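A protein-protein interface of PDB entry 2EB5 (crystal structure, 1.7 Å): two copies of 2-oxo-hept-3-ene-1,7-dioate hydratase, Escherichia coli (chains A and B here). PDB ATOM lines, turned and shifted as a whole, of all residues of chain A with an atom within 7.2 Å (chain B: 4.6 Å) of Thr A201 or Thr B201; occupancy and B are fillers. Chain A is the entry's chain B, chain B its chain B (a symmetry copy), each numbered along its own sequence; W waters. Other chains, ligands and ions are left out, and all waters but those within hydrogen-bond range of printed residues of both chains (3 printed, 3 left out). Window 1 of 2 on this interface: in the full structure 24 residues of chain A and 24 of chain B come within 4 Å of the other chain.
Leu A191 touches Val B203, and with the chains exchanged Val A203 touches Leu B191. Thr A201 touches Val B203, and with the chains exchanged Val A203 touches Thr B201. Thr A201 touches Phe B240, and with the chains exchanged Phe A240 touches Thr B201. Gly A202 touches Val B203, and with the chains exchanged Val A203 touches Gly B202. Of the 20 pairs that touch across the chains among the printed residues, 15 have their exchanged pair printed and touching as well.
The backbone carbonyl oxygen (O) of Val A107 lies within hydrogen-bond range of the backbone NH (N) of Phe A240, at 2.9 Å. O of Gly B202 lies within hydrogen-bond range of N of Ala B190, 3.0 Å away. N of Ala A190 lies within hydrogen-bond range of O of Gly A202 (3.0 Å).
Of the 19 printed residues of chain A, 11 touch a printed residue of chain B. Along chain A the printed residues that touch a printed residue of chain B span positions 69 to 242. Printed residues of chain B that touch a printed residue of chain A: Ala B190, Leu B191, Ile B198, Glu B200, Thr B201, Gly B202, Val B203, Gly B206 and Phe B240.
NH2 of Arg A242 lies within salt-bridge range of OE2 of Glu B200 (2.7 Å). N of Val A203 sits at hydrogen-bond distance from OG1 of Thr B201, 2.8 Å away. The side-chain hydroxyl (OG1) of Thr A201 lies within hydrogen-bond range of the backbone NH (N) of Val B203 (2.8 Å).
Printed residues of chain B within 4 Å of Thr A201: Thr B201, Gly B202, Val B203, Gly B206 and Phe B240. Of the printed residues of chain B, Phe A240 touches Thr B201 (3.9 Å). Of the printed residues of chain A, Ala B190 touches Val A203 (3.8 Å). Printed residues of chain A within 4 Å of Glu B200: Arg A242 (2.7 Å). Of chain A, only Thr A201, Gly A202, Val A203, Gly A206 and Phe A240 come within 4 Å of Thr B201. Of the printed residues of chain A, Gly B202 touches Thr A201 and Val A203. The nearest printed residue of chain B that does not touch Val A203 is Val B203 (4.4 Å).
Among the printed residues, pairs that only touch across the chains: Thr A201 with Gly B202 (3.3 Å), Gly A202 with Thr B201 (3.3 Å), Ala A205 with Ile B198 (3.5 Å), Gly A202 with Val B203 (3.6 Å), Val A203 with Gly B202 (3.6 Å), Val A203 with Leu B191 (3.6 Å), Leu A191 with Val B203 (3.6 Å), Thr A201 with Thr B201 (3.8 Å), Ser A189 with Val B203 (3.8 Å), Ala A205 with Leu B191 (3.8 Å), Thr A201 with Gly B206 (3.8 Å), Gly A206 with Thr B201 (3.8 Å), Ala A190 with Val B203 (3.8 Å), Val A203 with Ala B190 (3.8 Å), Phe A240 with Thr B201 (3.9 Å), Thr A201 with Phe B240 (3.9 Å) and Met A69 with Ile B198 (3.98 Å).
Water W1 lies within hydrogen-bond range of O of Phe B240 (2.7 Å) and OG1 of Thr A201 (2.7 Å). Water W2 bridges the backbone carbonyl oxygen (O) of Phe A240 (2.7 Å) and the side-chain hydroxyl (OG1) of Thr B201 (2.7 Å). Water W3 lies within hydrogen-bond range of O of Ile A198 and O of Gly B206.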
ATOM      1  N   MET A  69     -16.507 -10.653  -1.922  1.00  0.00           N
ATOM      2  CA  MET A  69     -16.179  -9.312  -2.464  1.00  0.00           C
ATOM      3  C   MET A  69     -15.016  -8.588  -1.770  1.00  0.00           C
ATOM      4  O   MET A  69     -14.225  -7.920  -2.432  1.00  0.00           O
ATOM      5  CB  MET A  69     -17.395  -8.388  -2.426  1.00  0.00           C
ATOM      6  CG  MET A  69     -18.613  -8.894  -3.152  1.00  0.00           C
ATOM      7  SD  MET A  69     -20.037  -8.035  -2.491  1.00  0.00           S
ATOM      8  CE  MET A  69     -19.941  -6.439  -3.344  1.00  0.00           C
ATOM      9  N   VAL A 107     -29.142  -9.687   7.468  1.00  0.00           N
ATOM     10  CA  VAL A 107     -30.150  -8.891   6.758  1.00  0.00           C
ATOM     11  C   VAL A 107     -30.053  -9.088   5.248  1.00  0.00           C
ATOM     12  O   VAL A 107     -29.014  -8.804   4.666  1.00  0.00           O
ATOM     13  CB  VAL A 107     -29.988  -7.376   7.123  1.00  0.00           C
ATOM     14  CG1 VAL A 107     -31.034  -6.528   6.369  1.00  0.00           C
ATOM     15  CG2 VAL A 107     -30.183  -7.201   8.611  1.00  0.00           C
ATOM     16  N   SER A 189     -32.225  -0.315   1.581  1.00  0.00           N
ATOM     17  CA  SER A 189     -31.307  -0.238   2.686  1.00  0.00           C
ATOM     18  C   SER A 189     -32.031  -0.595   3.995  1.00  0.00           C
ATOM     19  O   SER A 189     -33.269  -0.630   4.025  1.00  0.00           O
ATOM     20  CB  SER A 189     -30.686   1.156   2.720  1.00  0.00           C
ATOM     21  OG  SER A 189     -31.659   2.120   2.990  1.00  0.00           O
ATOM     22  N   ALA A 190     -31.272  -0.903   5.049  1.00  0.00           N
ATOM     23  CA  ALA A 190     -31.850  -1.385   6.302  1.00  0.00           C
ATOM     24  C   ALA A 190     -31.053  -0.952   7.517  1.00  0.00           C
ATOM     25  O   ALA A 190     -29.822  -0.783   7.466  1.00  0.00           O
ATOM     26  CB  ALA A 190     -31.968  -2.916   6.323  1.00  0.00           C
ATOM     27  N   LEU A 191     -31.776  -0.830   8.626  1.00  0.00           N
ATOM     28  CA  LEU A 191     -31.195  -0.608   9.936  1.00  0.00           C
ATOM     29  C   LEU A 191     -31.536  -1.816  10.785  1.00  0.00           C
ATOM     30  O   LEU A 191     -32.713  -2.109  10.971  1.00  0.00           O
ATOM     31  CB  LEU A 191     -31.822   0.626  10.613  1.00  0.00           C
ATOM     32  CG  LEU A 191     -31.973   1.848   9.719  1.00  0.00           C
ATOM     33  CD1 LEU A 191     -32.791   2.942  10.419  1.00  0.00           C
ATOM     34  CD2 LEU A 191     -30.588   2.419   9.241  1.00  0.00           C
ATOM     35  N   MET A 192     -30.515  -2.514  11.287  1.00  0.00           N
ATOM     36  CA  MET A 192     -30.764  -3.644  12.181  1.00  0.00           C
ATOM     37  C   MET A 192     -30.672  -3.212  13.640  1.00  0.00           C
ATOM     38  O   MET A 192     -29.578  -2.921  14.143  1.00  0.00           O
ATOM     39  CB  MET A 192     -29.799  -4.809  11.980  1.00  0.00           C
ATOM     40  CG  MET A 192     -30.200  -5.961  12.937  1.00  0.00           C
ATOM     41  SD  MET A 192     -28.869  -7.094  13.277  1.00  0.00           S
ATOM     42  CE  MET A 192     -28.163  -7.483  11.663  1.00  0.00           C
ATOM     43  N   ILE A 198     -29.407   0.371  17.214  1.00  0.00           N
ATOM     44  CA  ILE A 198     -28.955  -0.029  15.879  1.00  0.00           C
ATOM     45  C   ILE A 198     -27.559  -0.623  15.999  1.00  0.00           C
ATOM     46  O   ILE A 198     -26.610   0.066  16.424  1.00  0.00           O
ATOM     47  CB  ILE A 198     -28.915   1.178  14.908  1.00  0.00           C
ATOM     48  CG1 ILE A 198     -30.330   1.716  14.662  1.00  0.00           C
ATOM     49  CG2 ILE A 198     -28.219   0.807  13.593  1.00  0.00           C
ATOM     50  CD1 ILE A 198     -30.316   3.080  13.915  1.00  0.00           C
ATOM     51  N   GLU A 199     -27.451  -1.887  15.618  1.00  0.00           N
ATOM     52  CA  GLU A 199     -26.184  -2.637  15.665  1.00  0.00           C
ATOM     53  C   GLU A 199     -25.459  -2.661  14.338  1.00  0.00           C
ATOM     54  O   GLU A 199     -24.213  -2.708  14.318  1.00  0.00           O
ATOM     55  CB  GLU A 199     -26.415  -4.068  16.149  1.00  0.00           C
ATOM     56  CG  GLU A 199     -26.763  -4.132  17.651  1.00  0.00           C
ATOM     57  CD  GLU A 199     -25.583  -3.872  18.579  1.00  0.00           C
ATOM     58  OE1 GLU A 199     -24.416  -3.822  18.125  1.00  0.00           O
ATOM     59  OE2 GLU A 199     -25.841  -3.739  19.782  1.00  0.00           O
ATOM     60  N   GLU A 200     -26.213  -2.662  13.238  1.00  0.00           N
ATOM     61  CA  GLU A 200     -25.631  -2.661  11.877  1.00  0.00           C
ATOM     62  C   GLU A 200     -26.551  -1.919  10.949  1.00  0.00           C
ATOM     63  O   GLU A 200     -27.773  -1.921  11.149  1.00  0.00           O
ATOM     64  CB  GLU A 200     -25.456  -4.087  11.305  1.00  0.00           C
ATOM     65  CG  GLU A 200     -24.462  -5.011  12.067  1.00  0.00           C
ATOM     66  CD  GLU A 200     -23.010  -4.547  12.009  1.00  0.00           C
ATOM     67  OE1 GLU A 200     -22.634  -3.787  11.089  1.00  0.00           O
ATOM     68  OE2 GLU A 200     -22.222  -4.950  12.905  1.00  0.00           O
ATOM     69  N   THR A 201     -25.971  -1.331   9.908  1.00  0.00           N
ATOM     70  CA  THR A 201     -26.786  -0.815   8.787  1.00  0.00           C
ATOM     71  C   THR A 201     -26.172  -1.321   7.497  1.00  0.00           C
ATOM     72  O   THR A 201     -25.011  -1.758   7.477  1.00  0.00           O
ATOM     73  CB  THR A 201     -26.869   0.741   8.784  1.00  0.00           C
ATOM     74  OG1 THR A 201     -25.580   1.295   8.480  1.00  0.00           O
ATOM     75  CG2 THR A 201     -27.331   1.292  10.175  1.00  0.00           C
ATOM     76  N   GLY A 202     -26.924  -1.277   6.408  1.00  0.00           N
ATOM     77  CA  GLY A 202     -26.369  -1.743   5.159  1.00  0.00           C
ATOM     78  C   GLY A 202     -27.228  -1.366   3.976  1.00  0.00           C
ATOM     79  O   GLY A 202     -28.361  -0.942   4.149  1.00  0.00           O
ATOM     80  N   VAL A 203     -26.668  -1.498   2.771  1.00  0.00           N
ATOM     81  CA  VAL A 203     -27.420  -1.251   1.541  1.00  0.00           C
ATOM     82  C   VAL A 203     -27.299  -2.481   0.644  1.00  0.00           C
ATOM     83  O   VAL A 203     -26.221  -3.090   0.571  1.00  0.00           O
ATOM     84  CB  VAL A 203     -26.860   0.020   0.803  1.00  0.00           C
ATOM     85  CG1 VAL A 203     -27.753   0.437  -0.399  1.00  0.00           C
ATOM     86  CG2 VAL A 203     -26.680   1.185   1.806  1.00  0.00           C
ATOM     87  N   ALA A 204     -28.388  -2.826  -0.063  1.00  0.00           N
ATOM     88  CA  ALA A 204     -28.471  -4.107  -0.791  1.00  0.00           C
ATOM     89  C   ALA A 204     -27.419  -4.273  -1.905  1.00  0.00           C
ATOM     90  O   ALA A 204     -27.071  -5.404  -2.234  1.00  0.00           O
ATOM     91  CB  ALA A 204     -29.844  -4.338  -1.324  1.00  0.00           C
ATOM     92  N   ALA A 205     -26.889  -3.172  -2.449  1.00  0.00           N
ATOM     93  CA  ALA A 205     -25.826  -3.275  -3.465  1.00  0.00           C
ATOM     94  C   ALA A 205     -24.582  -3.953  -2.893  1.00  0.00           C
ATOM     95  O   ALA A 205     -23.775  -4.490  -3.638  1.00  0.00           O
ATOM     96  CB  ALA A 205     -25.479  -1.892  -4.070  1.00  0.00           C
ATOM     97  N   GLY A 206     -24.461  -3.970  -1.565  1.00  0.00           N
ATOM     98  CA  GLY A 206     -23.366  -4.678  -0.870  1.00  0.00           C
ATOM     99  C   GLY A 206     -23.329  -6.191  -1.129  1.00  0.00           C
ATOM    100  O   GLY A 206     -22.323  -6.862  -0.847  1.00  0.00           O
ATOM    101  N   VAL A 207     -24.426  -6.718  -1.656  1.00  0.00           N
ATOM    102  CA  VAL A 207     -24.522  -8.124  -2.089  1.00  0.00           C
ATOM    103  C   VAL A 207     -24.157  -8.206  -3.584  1.00  0.00           C
ATOM    104  O   VAL A 207     -25.013  -8.018  -4.478  1.00  0.00           O
ATOM    105  CB  VAL A 207     -25.943  -8.670  -1.862  1.00  0.00           C
ATOM    106  CG1 VAL A 207     -26.062 -10.126  -2.304  1.00  0.00           C
ATOM    107  CG2 VAL A 207     -26.369  -8.474  -0.399  1.00  0.00           C
ATOM    108  N   PHE A 240     -26.405  -8.182   3.528  1.00  0.00           N
ATOM    109  CA  PHE A 240     -25.684  -6.919   3.344  1.00  0.00           C
ATOM    110  C   PHE A 240     -25.271  -6.244   4.658  1.00  0.00           C
ATOM    111  O   PHE A 240     -24.762  -5.120   4.655  1.00  0.00           O
ATOM    112  CB  PHE A 240     -26.373  -5.966   2.364  1.00  0.00           C
ATOM    113  CG  PHE A 240     -27.854  -5.725   2.606  1.00  0.00           C
ATOM    114  CD1 PHE A 240     -28.269  -4.603   3.304  1.00  0.00           C
ATOM    115  CD2 PHE A 240     -28.827  -6.555   2.031  1.00  0.00           C
ATOM    116  CE1 PHE A 240     -29.626  -4.324   3.480  1.00  0.00           C
ATOM    117  CE2 PHE A 240     -30.194  -6.271   2.176  1.00  0.00           C
ATOM    118  CZ  PHE A 240     -30.583  -5.157   2.906  1.00  0.00           C
ATOM    119  N   THR A 241     -25.435  -6.974   5.766  1.00  0.00           N
ATOM    120  CA  THR A 241     -24.849  -6.584   7.053  1.00  0.00           C
ATOM    121  C   THR A 241     -24.016  -7.753   7.618  1.00  0.00           C
ATOM    122  O   THR A 241     -24.207  -8.935   7.251  1.00  0.00           O
ATOM    123  CB  THR A 241     -25.942  -6.231   8.121  1.00  0.00           C
ATOM    124  OG1 THR A 241     -26.732  -7.417   8.373  1.00  0.00           O
ATOM    125  CG2 THR A 241     -26.848  -5.107   7.617  1.00  0.00           C
ATOM    126  N   ARG A 242     -23.115  -7.433   8.534  1.00  0.00           N
ATOM    127  CA  ARG A 242     -22.464  -8.474   9.302  1.00  0.00           C
ATOM    128  C   ARG A 242     -23.516  -9.088  10.238  1.00  0.00           C
ATOM    129  O   ARG A 242     -24.475  -8.413  10.604  1.00  0.00           O
ATOM    130  CB  ARG A 242     -21.318  -7.907  10.105  1.00  0.00           C
ATOM    131  CG  ARG A 242     -20.176  -7.436   9.201  1.00  0.00           C
ATOM    132  CD  ARG A 242     -19.190  -6.617  10.024  1.00  0.00           C
ATOM    133  NE  ARG A 242     -17.972  -6.352   9.263  1.00  0.00           N
ATOM    134  CZ  ARG A 242     -17.841  -5.397   8.338  1.00  0.00           C
ATOM    135  NH1 ARG A 242     -18.869  -4.590   8.044  1.00  0.00           N
ATOM    136  NH2 ARG A 242     -16.668  -5.240   7.717  1.00  0.00           N
ATOM    137  N   ALA B 190     -24.882   5.063   1.730  1.00  0.00           N
ATOM    138  CA  ALA B 190     -23.668   5.109   0.917  1.00  0.00           C
ATOM    139  C   ALA B 190     -23.090   3.733   0.654  1.00  0.00           C
ATOM    140  O   ALA B 190     -23.213   2.804   1.472  1.00  0.00           O
ATOM    141  CB  ALA B 190     -22.579   5.974   1.568  1.00  0.00           C
ATOM    142  N   LEU B 191     -22.407   3.640  -0.482  1.00  0.00           N
ATOM    143  CA  LEU B 191     -21.619   2.476  -0.846  1.00  0.00           C
ATOM    144  C   LEU B 191     -20.175   2.928  -0.931  1.00  0.00           C
ATOM    145  O   LEU B 191     -19.867   3.817  -1.719  1.00  0.00           O
ATOM    146  CB  LEU B 191     -22.024   1.951  -2.236  1.00  0.00           C
ATOM    147  CG  LEU B 191     -23.521   1.861  -2.483  1.00  0.00           C
ATOM    148  CD1 LEU B 191     -23.816   1.530  -3.953  1.00  0.00           C
ATOM    149  CD2 LEU B 191     -24.228   0.823  -1.535  1.00  0.00           C
ATOM    150  N   ILE B 198     -17.095  -2.832  -3.755  1.00  0.00           N
ATOM    151  CA  ILE B 198     -17.750  -2.293  -2.560  1.00  0.00           C
ATOM    152  C   ILE B 198     -17.210  -3.028  -1.342  1.00  0.00           C
ATOM    153  O   ILE B 198     -17.369  -4.259  -1.220  1.00  0.00           O
ATOM    154  CB  ILE B 198     -19.288  -2.473  -2.626  1.00  0.00           C
ATOM    155  CG1 ILE B 198     -19.877  -1.636  -3.768  1.00  0.00           C
ATOM    156  CG2 ILE B 198     -19.942  -2.131  -1.283  1.00  0.00           C
ATOM    157  CD1 ILE B 198     -21.367  -1.986  -4.042  1.00  0.00           C
ATOM    158  N   GLU B 200     -17.700  -1.576   2.011  1.00  0.00           N
ATOM    159  CA  GLU B 200     -18.652  -1.323   3.118  1.00  0.00           C
ATOM    160  C   GLU B 200     -19.857  -0.607   2.574  1.00  0.00           C
ATOM    161  O   GLU B 200     -19.745   0.155   1.606  1.00  0.00           O
ATOM    162  CB  GLU B 200     -18.050  -0.430   4.227  1.00  0.00           C
ATOM    163  CG  GLU B 200     -16.832  -1.024   4.994  1.00  0.00           C
ATOM    164  CD  GLU B 200     -17.163  -2.257   5.829  1.00  0.00           C
ATOM    165  OE1 GLU B 200     -18.341  -2.467   6.194  1.00  0.00           O
ATOM    166  OE2 GLU B 200     -16.223  -3.040   6.129  1.00  0.00           O
ATOM    167  N   THR B 201     -20.994  -0.813   3.229  1.00  0.00           N
ATOM    168  CA  THR B 201     -22.174   0.040   2.970  1.00  0.00           C
ATOM    169  C   THR B 201     -22.718   0.498   4.309  1.00  0.00           C
ATOM    170  O   THR B 201     -22.395  -0.083   5.356  1.00  0.00           O
ATOM    171  CB  THR B 201     -23.274  -0.705   2.155  1.00  0.00           C
ATOM    172  OG1 THR B 201     -23.846  -1.750   2.956  1.00  0.00           O
ATOM    173  CG2 THR B 201     -22.687  -1.342   0.851  1.00  0.00           C
ATOM    174  N   GLY B 202     -23.542   1.534   4.307  1.00  0.00           N
ATOM    175  CA  GLY B 202     -24.086   1.994   5.565  1.00  0.00           C
ATOM    176  C   GLY B 202     -25.213   2.979   5.372  1.00  0.00           C
ATOM    177  O   GLY B 202     -25.418   3.474   4.275  1.00  0.00           O
ATOM    178  N   VAL B 203     -25.960   3.240   6.448  1.00  0.00           N
ATOM    179  CA  VAL B 203     -27.028   4.242   6.420  1.00  0.00           C
ATOM    180  C   VAL B 203     -26.795   5.228   7.561  1.00  0.00           C
ATOM    181  O   VAL B 203     -26.390   4.820   8.660  1.00  0.00           O
ATOM    182  CB  VAL B 203     -28.431   3.549   6.574  1.00  0.00           C
ATOM    183  CG1 VAL B 203     -29.602   4.547   6.348  1.00  0.00           C
ATOM    184  CG2 VAL B 203     -28.535   2.331   5.623  1.00  0.00           C
ATOM    185  N   GLY B 206     -27.241   5.076  11.424  1.00  0.00           N
ATOM    186  CA  GLY B 206     -26.222   4.333  12.193  1.00  0.00           C
ATOM    187  C   GLY B 206     -25.339   5.215  13.088  1.00  0.00           C
ATOM    188  O   GLY B 206     -24.641   4.717  13.986  1.00  0.00           O
ATOM    189  N   PHE B 240     -20.712   6.143   9.505  1.00  0.00           N
ATOM    190  CA  PHE B 240     -21.713   5.071   9.495  1.00  0.00           C
ATOM    191  C   PHE B 240     -21.245   3.792   8.791  1.00  0.00           C
ATOM    192  O   PHE B 240     -22.025   2.854   8.607  1.00  0.00           O
ATOM    193  CB  PHE B 240     -23.098   5.541   9.041  1.00  0.00           C
ATOM    194  CG  PHE B 240     -23.133   6.341   7.748  1.00  0.00           C
ATOM    195  CD1 PHE B 240     -23.438   5.713   6.552  1.00  0.00           C
ATOM    196  CD2 PHE B 240     -22.983   7.735   7.755  1.00  0.00           C
ATOM    197  CE1 PHE B 240     -23.545   6.439   5.364  1.00  0.00           C
ATOM    198  CE2 PHE B 240     -23.115   8.479   6.572  1.00  0.00           C
ATOM    199  CZ  PHE B 240     -23.391   7.822   5.382  1.00  0.00           C
ATOM    200  N   THR B 241     -19.949   3.745   8.465  1.00  0.00           N
ATOM    201  CA  THR B 241     -19.295   2.504   8.037  1.00  0.00           C
ATOM    202  C   THR B 241     -18.049   2.246   8.910  1.00  0.00           C
ATOM    203  O   THR B 241     -17.482   3.172   9.537  1.00  0.00           O
ATOM    204  CB  THR B 241     -18.813   2.571   6.546  1.00  0.00           C
ATOM    205  OG1 THR B 241     -17.820   3.617   6.435  1.00  0.00           O
ATOM    206  CG2 THR B 241     -19.986   2.872   5.612  1.00  0.00           C
HETATM  207  O   HOH W   1     -23.858   2.077  10.455  1.00  0.00           O
HETATM  208  O   HOH W   2     -22.950  -4.328   2.791  1.00  0.00           O
HETATM  209  O   HOH W   3     -24.663   1.759  15.039  1.00  0.00           O
